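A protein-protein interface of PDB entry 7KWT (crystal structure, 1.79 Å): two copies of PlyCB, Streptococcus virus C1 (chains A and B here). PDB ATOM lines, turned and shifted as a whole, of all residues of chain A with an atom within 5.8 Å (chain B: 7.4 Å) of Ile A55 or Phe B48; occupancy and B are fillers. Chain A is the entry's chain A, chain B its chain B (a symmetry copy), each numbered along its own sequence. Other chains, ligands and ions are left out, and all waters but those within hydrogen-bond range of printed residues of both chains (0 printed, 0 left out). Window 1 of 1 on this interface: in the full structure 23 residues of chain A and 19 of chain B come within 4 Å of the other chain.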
ATOM      1  N   PHE A  16       9.044 -28.919 -23.257  1.00  0.00           N
ATOM      2  CA  PHE A  16      10.239 -28.376 -23.886  1.00  0.00           C
ATOM      3  C   PHE A  16      10.852 -29.413 -24.812  1.00  0.00           C
ATOM      4  O   PHE A  16      10.674 -30.619 -24.624  1.00  0.00           O
ATOM      5  CB  PHE A  16      11.271 -27.919 -22.838  1.00  0.00           C
ATOM      6  CG  PHE A  16      11.665 -28.994 -21.851  1.00  0.00           C
ATOM      7  CD1 PHE A  16      12.675 -29.897 -22.148  1.00  0.00           C
ATOM      8  CD2 PHE A  16      11.031 -29.088 -20.620  1.00  0.00           C
ATOM      9  CE1 PHE A  16      13.031 -30.882 -21.246  1.00  0.00           C
ATOM     10  CE2 PHE A  16      11.387 -30.064 -19.710  1.00  0.00           C
ATOM     11  CZ  PHE A  16      12.392 -30.965 -20.024  1.00  0.00           C
ATOM     12  N   LEU A  17      11.566 -28.921 -25.820  1.00  0.00           N
ATOM     13  CA  LEU A  17      12.442 -29.757 -26.626  1.00  0.00           C
ATOM     14  C   LEU A  17      13.791 -29.878 -25.932  1.00  0.00           C
ATOM     15  O   LEU A  17      14.232 -28.956 -25.244  1.00  0.00           O
ATOM     16  CB  LEU A  17      12.639 -29.150 -28.013  1.00  0.00           C
ATOM     17  CG  LEU A  17      11.421 -29.104 -28.938  1.00  0.00           C
ATOM     18  CD1 LEU A  17      11.418 -27.818 -29.744  1.00  0.00           C
ATOM     19  CD2 LEU A  17      11.443 -30.310 -29.862  1.00  0.00           C
ATOM     20  N   PHE A  18      14.452 -31.022 -26.117  1.00  0.00           N
ATOM     21  CA  PHE A  18      15.789 -31.157 -25.560  1.00  0.00           C
ATOM     22  C   PHE A  18      16.666 -32.000 -26.475  1.00  0.00           C
ATOM     23  O   PHE A  18      16.192 -32.895 -27.181  1.00  0.00           O
ATOM     24  CB  PHE A  18      15.792 -31.724 -24.125  1.00  0.00           C
ATOM     25  CG  PHE A  18      15.179 -33.094 -23.972  1.00  0.00           C
ATOM     26  CD1 PHE A  18      13.805 -33.255 -23.924  1.00  0.00           C
ATOM     27  CD2 PHE A  18      15.987 -34.215 -23.804  1.00  0.00           C
ATOM     28  CE1 PHE A  18      13.243 -34.511 -23.756  1.00  0.00           C
ATOM     29  CE2 PHE A  18      15.434 -35.468 -23.630  1.00  0.00           C
ATOM     30  CZ  PHE A  18      14.054 -35.618 -23.607  1.00  0.00           C
ATOM     31  N   HIS A  19      17.955 -31.671 -26.463  1.00  0.00           N
ATOM     32  CA  HIS A  19      18.979 -32.369 -27.228  1.00  0.00           C
ATOM     33  C   HIS A  19      20.306 -32.114 -26.529  1.00  0.00           C
ATOM     34  O   HIS A  19      20.404 -31.250 -25.656  1.00  0.00           O
ATOM     35  CB  HIS A  19      19.022 -31.880 -28.680  1.00  0.00           C
ATOM     36  CG  HIS A  19      19.675 -30.541 -28.838  1.00  0.00           C
ATOM     37  ND1 HIS A  19      19.027 -29.358 -28.555  1.00  0.00           N
ATOM     38  CD2 HIS A  19      20.926 -30.198 -29.230  1.00  0.00           C
ATOM     39  CE1 HIS A  19      19.846 -28.345 -28.773  1.00  0.00           C
ATOM     40  NE2 HIS A  19      21.004 -28.826 -29.186  1.00  0.00           N
ATOM     41  N   PRO A  53       9.874 -23.944 -25.167  1.00  0.00           N
ATOM     42  CA  PRO A  53      11.322 -23.728 -25.116  1.00  0.00           C
ATOM     43  C   PRO A  53      12.095 -24.925 -25.643  1.00  0.00           C
ATOM     44  O   PRO A  53      11.601 -26.055 -25.697  1.00  0.00           O
ATOM     45  CB  PRO A  53      11.607 -23.516 -23.622  1.00  0.00           C
ATOM     46  CG  PRO A  53      10.299 -23.209 -23.004  1.00  0.00           C
ATOM     47  CD  PRO A  53       9.263 -23.910 -23.826  1.00  0.00           C
ATOM     48  N   SER A  54      13.339 -24.650 -26.030  1.00  0.00           N
ATOM     49  CA  SER A  54      14.271 -25.667 -26.508  1.00  0.00           C
ATOM     50  C   SER A  54      15.544 -25.544 -25.692  1.00  0.00           C
ATOM     51  O   SER A  54      16.207 -24.502 -25.734  1.00  0.00           O
ATOM     52  CB  SER A  54      14.580 -25.495 -27.999  1.00  0.00           C
ATOM     53  OG  SER A  54      15.293 -26.620 -28.487  1.00  0.00           O
ATOM     54  N   ILE A  55      15.887 -26.596 -24.944  1.00  0.00           N
ATOM     55  CA  ILE A  55      17.011 -26.521 -24.020  1.00  0.00           C
ATOM     56  C   ILE A  55      17.960 -27.685 -24.265  1.00  0.00           C
ATOM     57  O   ILE A  55      17.622 -28.671 -24.917  1.00  0.00           O
ATOM     58  CB  ILE A  55      16.560 -26.506 -22.544  1.00  0.00           C
ATOM     59  CG1 ILE A  55      15.854 -27.815 -22.181  1.00  0.00           C
ATOM     60  CG2 ILE A  55      15.663 -25.299 -22.270  1.00  0.00           C
ATOM     61  CD1 ILE A  55      15.604 -27.977 -20.679  1.00  0.00           C
ATOM     62  N   ASN A  56      19.165 -27.557 -23.717  1.00  0.00           N
ATOM     63  CA  ASN A  56      20.191 -28.589 -23.819  1.00  0.00           C
ATOM     64  C   ASN A  56      20.192 -29.446 -22.561  1.00  0.00           C
ATOM     65  O   ASN A  56      20.165 -28.919 -21.445  1.00  0.00           O
ATOM     66  CB  ASN A  56      21.574 -27.967 -24.010  1.00  0.00           C
ATOM     67  CG  ASN A  56      21.764 -27.381 -25.391  1.00  0.00           C
ATOM     68  OD1 ASN A  56      21.060 -26.459 -25.782  1.00  0.00           O
ATOM     69  ND2 ASN A  56      22.734 -27.907 -26.130  1.00  0.00           N
ATOM     70  N   ILE A  57      20.241 -30.765 -22.745  1.00  0.00           N
ATOM     71  CA  ILE A  57      20.322 -31.716 -21.639  1.00  0.00           C
ATOM     72  C   ILE A  57      21.353 -32.771 -22.014  1.00  0.00           C
ATOM     73  O   ILE A  57      21.240 -33.399 -23.072  1.00  0.00           O
ATOM     74  CB  ILE A  57      18.966 -32.379 -21.337  1.00  0.00           C
ATOM     75  CG1 ILE A  57      17.924 -31.320 -20.967  1.00  0.00           C
ATOM     76  CG2 ILE A  57      19.111 -33.407 -20.215  1.00  0.00           C
ATOM     77  CD1 ILE A  57      16.567 -31.893 -20.593  1.00  0.00           C
ATOM     78  N   ILE A  65      16.111 -36.258 -15.330  1.00  0.00           N
ATOM     79  CA  ILE A  65      15.046 -35.358 -15.765  1.00  0.00           C
ATOM     80  C   ILE A  65      13.743 -36.126 -15.962  1.00  0.00           C
ATOM     81  O   ILE A  65      12.660 -35.632 -15.630  1.00  0.00           O
ATOM     82  CB  ILE A  65      15.464 -34.608 -17.043  1.00  0.00           C
ATOM     83  CG1 ILE A  65      16.750 -33.809 -16.803  1.00  0.00           C
ATOM     84  CG2 ILE A  65      14.346 -33.688 -17.510  1.00  0.00           C
ATOM     85  CD1 ILE A  65      16.667 -32.861 -15.630  1.00  0.00           C
ATOM     86  N   SER B  11       6.810 -24.030 -20.072  1.00  0.00           N
ATOM     87  CA  SER B  11       7.805 -25.098 -20.041  1.00  0.00           C
ATOM     88  C   SER B  11       7.324 -26.334 -19.293  1.00  0.00           C
ATOM     89  O   SER B  11       7.917 -27.406 -19.450  1.00  0.00           O
ATOM     90  CB  SER B  11       9.098 -24.598 -19.397  1.00  0.00           C
ATOM     91  OG  SER B  11       8.957 -24.522 -17.988  1.00  0.00           O
ATOM     92  N   VAL B  13       7.741 -26.738 -16.196  1.00  0.00           N
ATOM     93  CA  VAL B  13       8.766 -26.967 -15.188  1.00  0.00           C
ATOM     94  C   VAL B  13       8.656 -25.866 -14.145  1.00  0.00           C
ATOM     95  O   VAL B  13       8.681 -24.680 -14.489  1.00  0.00           O
ATOM     96  CB  VAL B  13      10.177 -26.986 -15.806  1.00  0.00           C
ATOM     97  CG1 VAL B  13      11.238 -27.162 -14.717  1.00  0.00           C
ATOM     98  CG2 VAL B  13      10.291 -28.090 -16.856  1.00  0.00           C
ATOM     99  N   PHE B  16      13.924 -24.820  -9.142  1.00  0.00           N
ATOM    100  CA  PHE B  16      15.155 -24.048  -9.186  1.00  0.00           C
ATOM    101  C   PHE B  16      16.348 -24.987  -9.111  1.00  0.00           C
ATOM    102  O   PHE B  16      16.258 -26.091  -8.570  1.00  0.00           O
ATOM    103  CB  PHE B  16      15.211 -23.011  -8.046  1.00  0.00           C
ATOM    104  CG  PHE B  16      15.094 -23.605  -6.663  1.00  0.00           C
ATOM    105  CD1 PHE B  16      13.849 -23.819  -6.090  1.00  0.00           C
ATOM    106  CD2 PHE B  16      16.229 -23.937  -5.932  1.00  0.00           C
ATOM    107  CE1 PHE B  16      13.733 -24.358  -4.821  1.00  0.00           C
ATOM    108  CE2 PHE B  16      16.122 -24.478  -4.659  1.00  0.00           C
ATOM    109  CZ  PHE B  16      14.870 -24.688  -4.101  1.00  0.00           C
ATOM    110  N   LEU B  17      17.455 -24.534  -9.683  1.00  0.00           N
ATOM    111  CA  LEU B  17      18.752 -25.150  -9.481  1.00  0.00           C
ATOM    112  C   LEU B  17      19.378 -24.588  -8.213  1.00  0.00           C
ATOM    113  O   LEU B  17      19.155 -23.427  -7.860  1.00  0.00           O
ATOM    114  CB  LEU B  17      19.669 -24.870 -10.668  1.00  0.00           C
ATOM    115  CG  LEU B  17      19.258 -25.465 -12.015  1.00  0.00           C
ATOM    116  CD1 LEU B  17      19.526 -24.468 -13.126  1.00  0.00           C
ATOM    117  CD2 LEU B  17      20.015 -26.755 -12.263  1.00  0.00           C
ATOM    118  N   ALA B  30      18.762 -29.771  -8.298  1.00  0.00           N
ATOM    119  CA  ALA B  30      17.582 -28.997  -8.645  1.00  0.00           C
ATOM    120  C   ALA B  30      16.360 -29.611  -7.990  1.00  0.00           C
ATOM    121  O   ALA B  30      16.297 -30.822  -7.765  1.00  0.00           O
ATOM    122  CB  ALA B  30      17.364 -28.924 -10.163  1.00  0.00           C
ATOM    123  N   ILE B  32      12.705 -29.952  -9.332  1.00  0.00           N
ATOM    124  CA  ILE B  32      11.935 -29.834 -10.561  1.00  0.00           C
ATOM    125  C   ILE B  32      10.582 -30.470 -10.292  1.00  0.00           C
ATOM    126  O   ILE B  32      10.492 -31.687 -10.088  1.00  0.00           O
ATOM    127  CB  ILE B  32      12.641 -30.487 -11.757  1.00  0.00           C
ATOM    128  CG1 ILE B  32      13.927 -29.715 -12.076  1.00  0.00           C
ATOM    129  CG2 ILE B  32      11.714 -30.531 -12.971  1.00  0.00           C
ATOM    130  CD1 ILE B  32      14.708 -30.261 -13.238  1.00  0.00           C
ATOM    131  N   ILE B  37      16.726 -33.668  -7.694  1.00  0.00           N
ATOM    132  CA  ILE B  37      17.623 -34.479  -8.508  1.00  0.00           C
ATOM    133  C   ILE B  37      19.012 -33.862  -8.491  1.00  0.00           C
ATOM    134  O   ILE B  37      19.188 -32.670  -8.232  1.00  0.00           O
ATOM    135  CB  ILE B  37      17.145 -34.609  -9.972  1.00  0.00           C
ATOM    136  CG1 ILE B  37      17.009 -33.220 -10.600  1.00  0.00           C
ATOM    137  CG2 ILE B  37      15.839 -35.391 -10.051  1.00  0.00           C
ATOM    138  CD1 ILE B  37      16.699 -33.248 -12.074  1.00  0.00           C
ATOM    139  N   ILE B  39      22.340 -32.975 -10.861  1.00  0.00           N
ATOM    140  CA  ILE B  39      22.687 -32.660 -12.241  1.00  0.00           C
ATOM    141  C   ILE B  39      24.164 -32.962 -12.424  1.00  0.00           C
ATOM    142  O   ILE B  39      25.001 -32.472 -11.657  1.00  0.00           O
ATOM    143  CB  ILE B  39      22.381 -31.193 -12.589  1.00  0.00           C
ATOM    144  CG1 ILE B  39      20.944 -30.834 -12.209  1.00  0.00           C
ATOM    145  CG2 ILE B  39      22.643 -30.938 -14.067  1.00  0.00           C
ATOM    146  CD1 ILE B  39      19.900 -31.584 -12.989  1.00  0.00           C
ATOM    147  N   ILE B  42      27.516 -29.706 -16.949  1.00  0.00           N
ATOM    148  CA  ILE B  42      27.294 -28.266 -17.046  1.00  0.00           C
ATOM    149  C   ILE B  42      26.366 -27.920 -18.204  1.00  0.00           C
ATOM    150  O   ILE B  42      25.660 -26.905 -18.154  1.00  0.00           O
ATOM    151  CB  ILE B  42      28.643 -27.529 -17.166  1.00  0.00           C
ATOM    152  CG1 ILE B  42      28.445 -26.024 -16.972  1.00  0.00           C
ATOM    153  CG2 ILE B  42      29.291 -27.818 -18.502  1.00  0.00           C
ATOM    154  CD1 ILE B  42      27.930 -25.651 -15.602  1.00  0.00           C
ATOM    155  N   GLU B  43      26.349 -28.736 -19.264  1.00  0.00           N
ATOM    156  CA  GLU B  43      25.413 -28.470 -20.354  1.00  0.00           C
ATOM    157  C   GLU B  43      23.982 -28.460 -19.846  1.00  0.00           C
ATOM    158  O   GLU B  43      23.182 -27.595 -20.226  1.00  0.00           O
ATOM    159  CB  GLU B  43      25.572 -29.504 -21.473  1.00  0.00           C
ATOM    160  CG  GLU B  43      24.484 -29.399 -22.546  1.00  0.00           C
ATOM    161  CD  GLU B  43      24.638 -30.424 -23.664  1.00  0.00           C
ATOM    162  OE1 GLU B  43      24.970 -31.593 -23.367  1.00  0.00           O
ATOM    163  OE2 GLU B  43      24.420 -30.061 -24.839  1.00  0.00           O
ATOM    164  N   THR B  44      23.646 -29.413 -18.971  1.00  0.00           N
ATOM    165  CA  THR B  44      22.293 -29.498 -18.433  1.00  0.00           C
ATOM    166  C   THR B  44      21.993 -28.324 -17.510  1.00  0.00           C
ATOM    167  O   THR B  44      20.872 -27.800 -17.506  1.00  0.00           O
ATOM    168  CB  THR B  44      22.116 -30.820 -17.685  1.00  0.00           C
ATOM    169  OG1 THR B  44      22.514 -31.909 -18.534  1.00  0.00           O
ATOM    170  CG2 THR B  44      20.661 -31.012 -17.261  1.00  0.00           C
ATOM    171  N   VAL B  45      22.978 -27.908 -16.713  1.00  0.00           N
ATOM    172  CA  VAL B  45      22.794 -26.742 -15.852  1.00  0.00           C
ATOM    173  C   VAL B  45      22.447 -25.521 -16.691  1.00  0.00           C
ATOM    174  O   VAL B  45      21.471 -24.813 -16.418  1.00  0.00           O
ATOM    175  CB  VAL B  45      24.058 -26.495 -15.009  1.00  0.00           C
ATOM    176  CG1 VAL B  45      23.966 -25.147 -14.301  1.00  0.00           C
ATOM    177  CG2 VAL B  45      24.255 -27.614 -14.003  1.00  0.00           C
ATOM    178  N   GLN B  46      23.242 -25.262 -17.732  1.00  0.00           N
ATOM    179  CA  GLN B  46      23.003 -24.089 -18.566  1.00  0.00           C
ATOM    180  C   GLN B  46      21.703 -24.215 -19.347  1.00  0.00           C
ATOM    181  O   GLN B  46      21.027 -23.206 -19.588  1.00  0.00           O
ATOM    182  CB  GLN B  46      24.198 -23.856 -19.494  1.00  0.00           C
ATOM    183  CG  GLN B  46      25.467 -23.488 -18.714  1.00  0.00           C
ATOM    184  CD  GLN B  46      26.577 -22.897 -19.572  1.00  0.00           C
ATOM    185  OE1 GLN B  46      26.967 -23.465 -20.587  1.00  0.00           O
ATOM    186  NE2 GLN B  46      27.095 -21.749 -19.151  1.00  0.00           N
ATOM    187  N   GLY B  47      21.319 -25.437 -19.721  1.00  0.00           N
ATOM    188  CA  GLY B  47      20.027 -25.618 -20.369  1.00  0.00           C
ATOM    189  C   GLY B  47      18.877 -25.237 -19.456  1.00  0.00           C
ATOM    190  O   GLY B  47      17.985 -24.474 -19.839  1.00  0.00           O
ATOM    191  N   PHE B  48      18.890 -25.743 -18.220  1.00  0.00           N
ATOM    192  CA  PHE B  48      17.788 -25.418 -17.324  1.00  0.00           C
ATOM    193  C   PHE B  48      17.849 -23.986 -16.817  1.00  0.00           C
ATOM    194  O   PHE B  48      16.806 -23.432 -16.449  1.00  0.00           O
ATOM    195  CB  PHE B  48      17.734 -26.413 -16.165  1.00  0.00           C
ATOM    196  CG  PHE B  48      16.956 -27.651 -16.505  1.00  0.00           C
ATOM    197  CD1 PHE B  48      15.592 -27.709 -16.287  1.00  0.00           C
ATOM    198  CD2 PHE B  48      17.580 -28.729 -17.112  1.00  0.00           C
ATOM    199  CE1 PHE B  48      14.867 -28.837 -16.630  1.00  0.00           C
ATOM    200  CE2 PHE B  48      16.859 -29.861 -17.460  1.00  0.00           C
ATOM    201  CZ  PHE B  48      15.503 -29.913 -17.215  1.00  0.00           C
ATOM    202  N   GLN B  49      19.026 -23.358 -16.834  1.00  0.00           N
ATOM    203  CA  GLN B  49      19.107 -21.944 -16.485  1.00  0.00           C
ATOM    204  C   GLN B  49      18.341 -21.066 -17.467  1.00  0.00           C
ATOM    205  O   GLN B  49      18.043 -19.910 -17.148  1.00  0.00           O
ATOM    206  CB  GLN B  49      20.572 -21.508 -16.400  1.00  0.00           C
ATOM    207  CG  GLN B  49      21.222 -21.888 -15.074  1.00  0.00           C
ATOM    208  CD  GLN B  49      22.716 -21.629 -15.036  1.00  0.00           C
ATOM    209  OE1 GLN B  49      23.361 -21.457 -16.071  1.00  0.00           O
ATOM    210  NE2 GLN B  49      23.276 -21.604 -13.830  1.00  0.00           N
ATOM    211  N   GLN B  50      17.983 -21.597 -18.637  1.00  0.00           N
ATOM    212  CA  GLN B  50      17.150 -20.838 -19.557  1.00  0.00           C
ATOM    213  C   GLN B  50      15.696 -20.773 -19.104  1.00  0.00           C
ATOM    214  O   GLN B  50      14.968 -19.873 -19.540  1.00  0.00           O
ATOM    215  CB  GLN B  50      17.237 -21.447 -20.959  1.00  0.00           C
ATOM    216  CG  GLN B  50      18.603 -21.287 -21.610  1.00  0.00           C
ATOM    217  CD  GLN B  50      18.915 -19.840 -21.945  1.00  0.00           C
ATOM    218  OE1 GLN B  50      18.191 -19.198 -22.709  1.00  0.00           O
ATOM    219  NE2 GLN B  50      19.990 -19.316 -21.369  1.00  0.00           N
ATOM    220  N   ILE B  51      15.259 -21.675 -18.226  1.00  0.00           N
ATOM    221  CA  ILE B  51      13.840 -21.746 -17.885  1.00  0.00           C
ATOM    222  C   ILE B  51      13.553 -21.719 -16.390  1.00  0.00           C
ATOM    223  O   ILE B  51      12.390 -21.486 -16.013  1.00  0.00           O
ATOM    224  CB  ILE B  51      13.173 -22.983 -18.532  1.00  0.00           C
ATOM    225  CG1 ILE B  51      13.880 -24.273 -18.116  1.00  0.00           C
ATOM    226  CG2 ILE B  51      13.138 -22.844 -20.053  1.00  0.00           C
ATOM    227  CD1 ILE B  51      13.070 -25.518 -18.415  1.00  0.00           C
ATOM    228  N   ILE B  52      14.508 -21.963 -15.493  1.00  0.00           N
ATOM    229  CA  ILE B  52      14.232 -21.862 -14.057  1.00  0.00           C
ATOM    230  C   ILE B  52      15.366 -21.100 -13.383  1.00  0.00           C
ATOM    231  O   ILE B  52      16.502 -21.069 -13.882  1.00  0.00           O
ATOM    232  CB  ILE B  52      14.044 -23.253 -13.404  1.00  0.00           C
ATOM    233  CG1 ILE B  52      15.209 -24.182 -13.766  1.00  0.00           C
ATOM    234  CG2 ILE B  52      12.699 -23.851 -13.798  1.00  0.00           C
ATOM    235  CD1 ILE B  52      15.288 -25.426 -12.903  1.00  0.00           C
ATOM    236  N   PRO B  53      15.093 -20.480 -12.235  1.00  0.00           N
ATOM    237  CA  PRO B  53      16.150 -19.743 -11.532  1.00  0.00           C
ATOM    238  C   PRO B  53      17.221 -20.665 -10.976  1.00  0.00           C
ATOM    239  O   PRO B  53      17.007 -21.857 -10.744  1.00  0.00           O
ATOM    240  CB  PRO B  53      15.403 -19.027 -10.397  1.00  0.00           C
ATOM    241  CG  PRO B  53      14.142 -19.802 -10.213  1.00  0.00           C
ATOM    242  CD  PRO B  53      13.781 -20.315 -11.586  1.00  0.00           C
ATOM    243  N   SER B  54      18.390 -20.075 -10.740  1.00  0.00           N
ATOM    244  CA  SER B  54      19.543 -20.782 -10.195  1.00  0.00           C
ATOM    245  C   SER B  54      20.054 -19.991  -8.998  1.00  0.00           C
ATOM    246  O   SER B  54      20.447 -18.830  -9.144  1.00  0.00           O
ATOM    247  CB  SER B  54      20.626 -20.945 -11.269  1.00  0.00           C
ATOM    248  OG  SER B  54      21.824 -21.462 -10.723  1.00  0.00           O
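OE2 of Glu B43 is in hydrogen-bond range of ND2 of Asn A56 (3.0 Å).
The backbone NH (N) of Leu A17 is in hydrogen-bond range of the backbone carbonyl oxygen (O) of Pro A53.
O of Leu A17 lies within hydrogen-bond range of N of Ile A55.
N of His A19 lies within hydrogen-bond range of O of Ile A55.
O of His A19 is in hydrogen-bond range of N of Ile A57 (3.0 Å).
The side-chain hydroxyl of Ser B11 lies within hydrogen-bond range of the backbone NH of Val B13.
N of Ile B37 sits at hydrogen-bond distance from O of Ala B30 (2.9 Å).
Phe A16 touches Val B13.
Pro A53 touches Ile B51.
Gly B47 touches Ile A55.
Ile A55 touches Phe B48 (CD1 to CE2, 3.9 Å).
Asn A56 touches Thr B44.
Asn A56 touches Gly B47 (O to CA, 3.5 Å).
Ile A57 touches Thr B44.
CD1 of Ile A57 touches CE2 of Phe B48 (3.7 Å).
Ile A65 touches Ile B37.
Ile A65 touches Phe B48 (CD1 to CE2, 3.5 Å).
Ile A55 touches two residues of chain B.
Printed residues of chain B within 4 Å of Ile A65: Ile B37 and Phe B48.
Printed residues of chain B within 4 Å of Phe A16: Ser B11 and Val B13.
Printed residues of chain B within 4 Å of Pro A53: Ile B51 (3.9 Å).
Of the printed residues of chain A, Ser B11 touches Phe A16.
Ser B54 touches none of the printed residues of chain A.
Leu A17 touches none of the printed residues of chain B.
The nearest residue of chain B that does not touch Ile A55 is Ile B51 (4.2 Å).
The nearest residue of chain A that does not touch Phe B48 is Phe A16 (4.3 Å).
The nearest printed residue of chain A that does not touch Glu B43 is Ile A57 (4.04 Å).
Hydrophobic or aromatic side chains of chain B that line the printed part of chain A: Val B13, Ile B37, Phe B48 and Ile B51.
Hydrophobic or aromatic side chains of chain A within 4 Å of the printed part of chain B: Phe A16, Pro A53, Ile A55, Ile A57 and Ile A65.
Among the printed residues, no Asp or Glu carboxylate lies within 4 Å of a Lys or Arg side-chain nitrogen of the other chain.
Positions printed for both chains: 16, 17, 53 and 54.
Of the 12 pairs that touch across the chains among the printed residues, none has its exchanged pair printed and touching as well.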
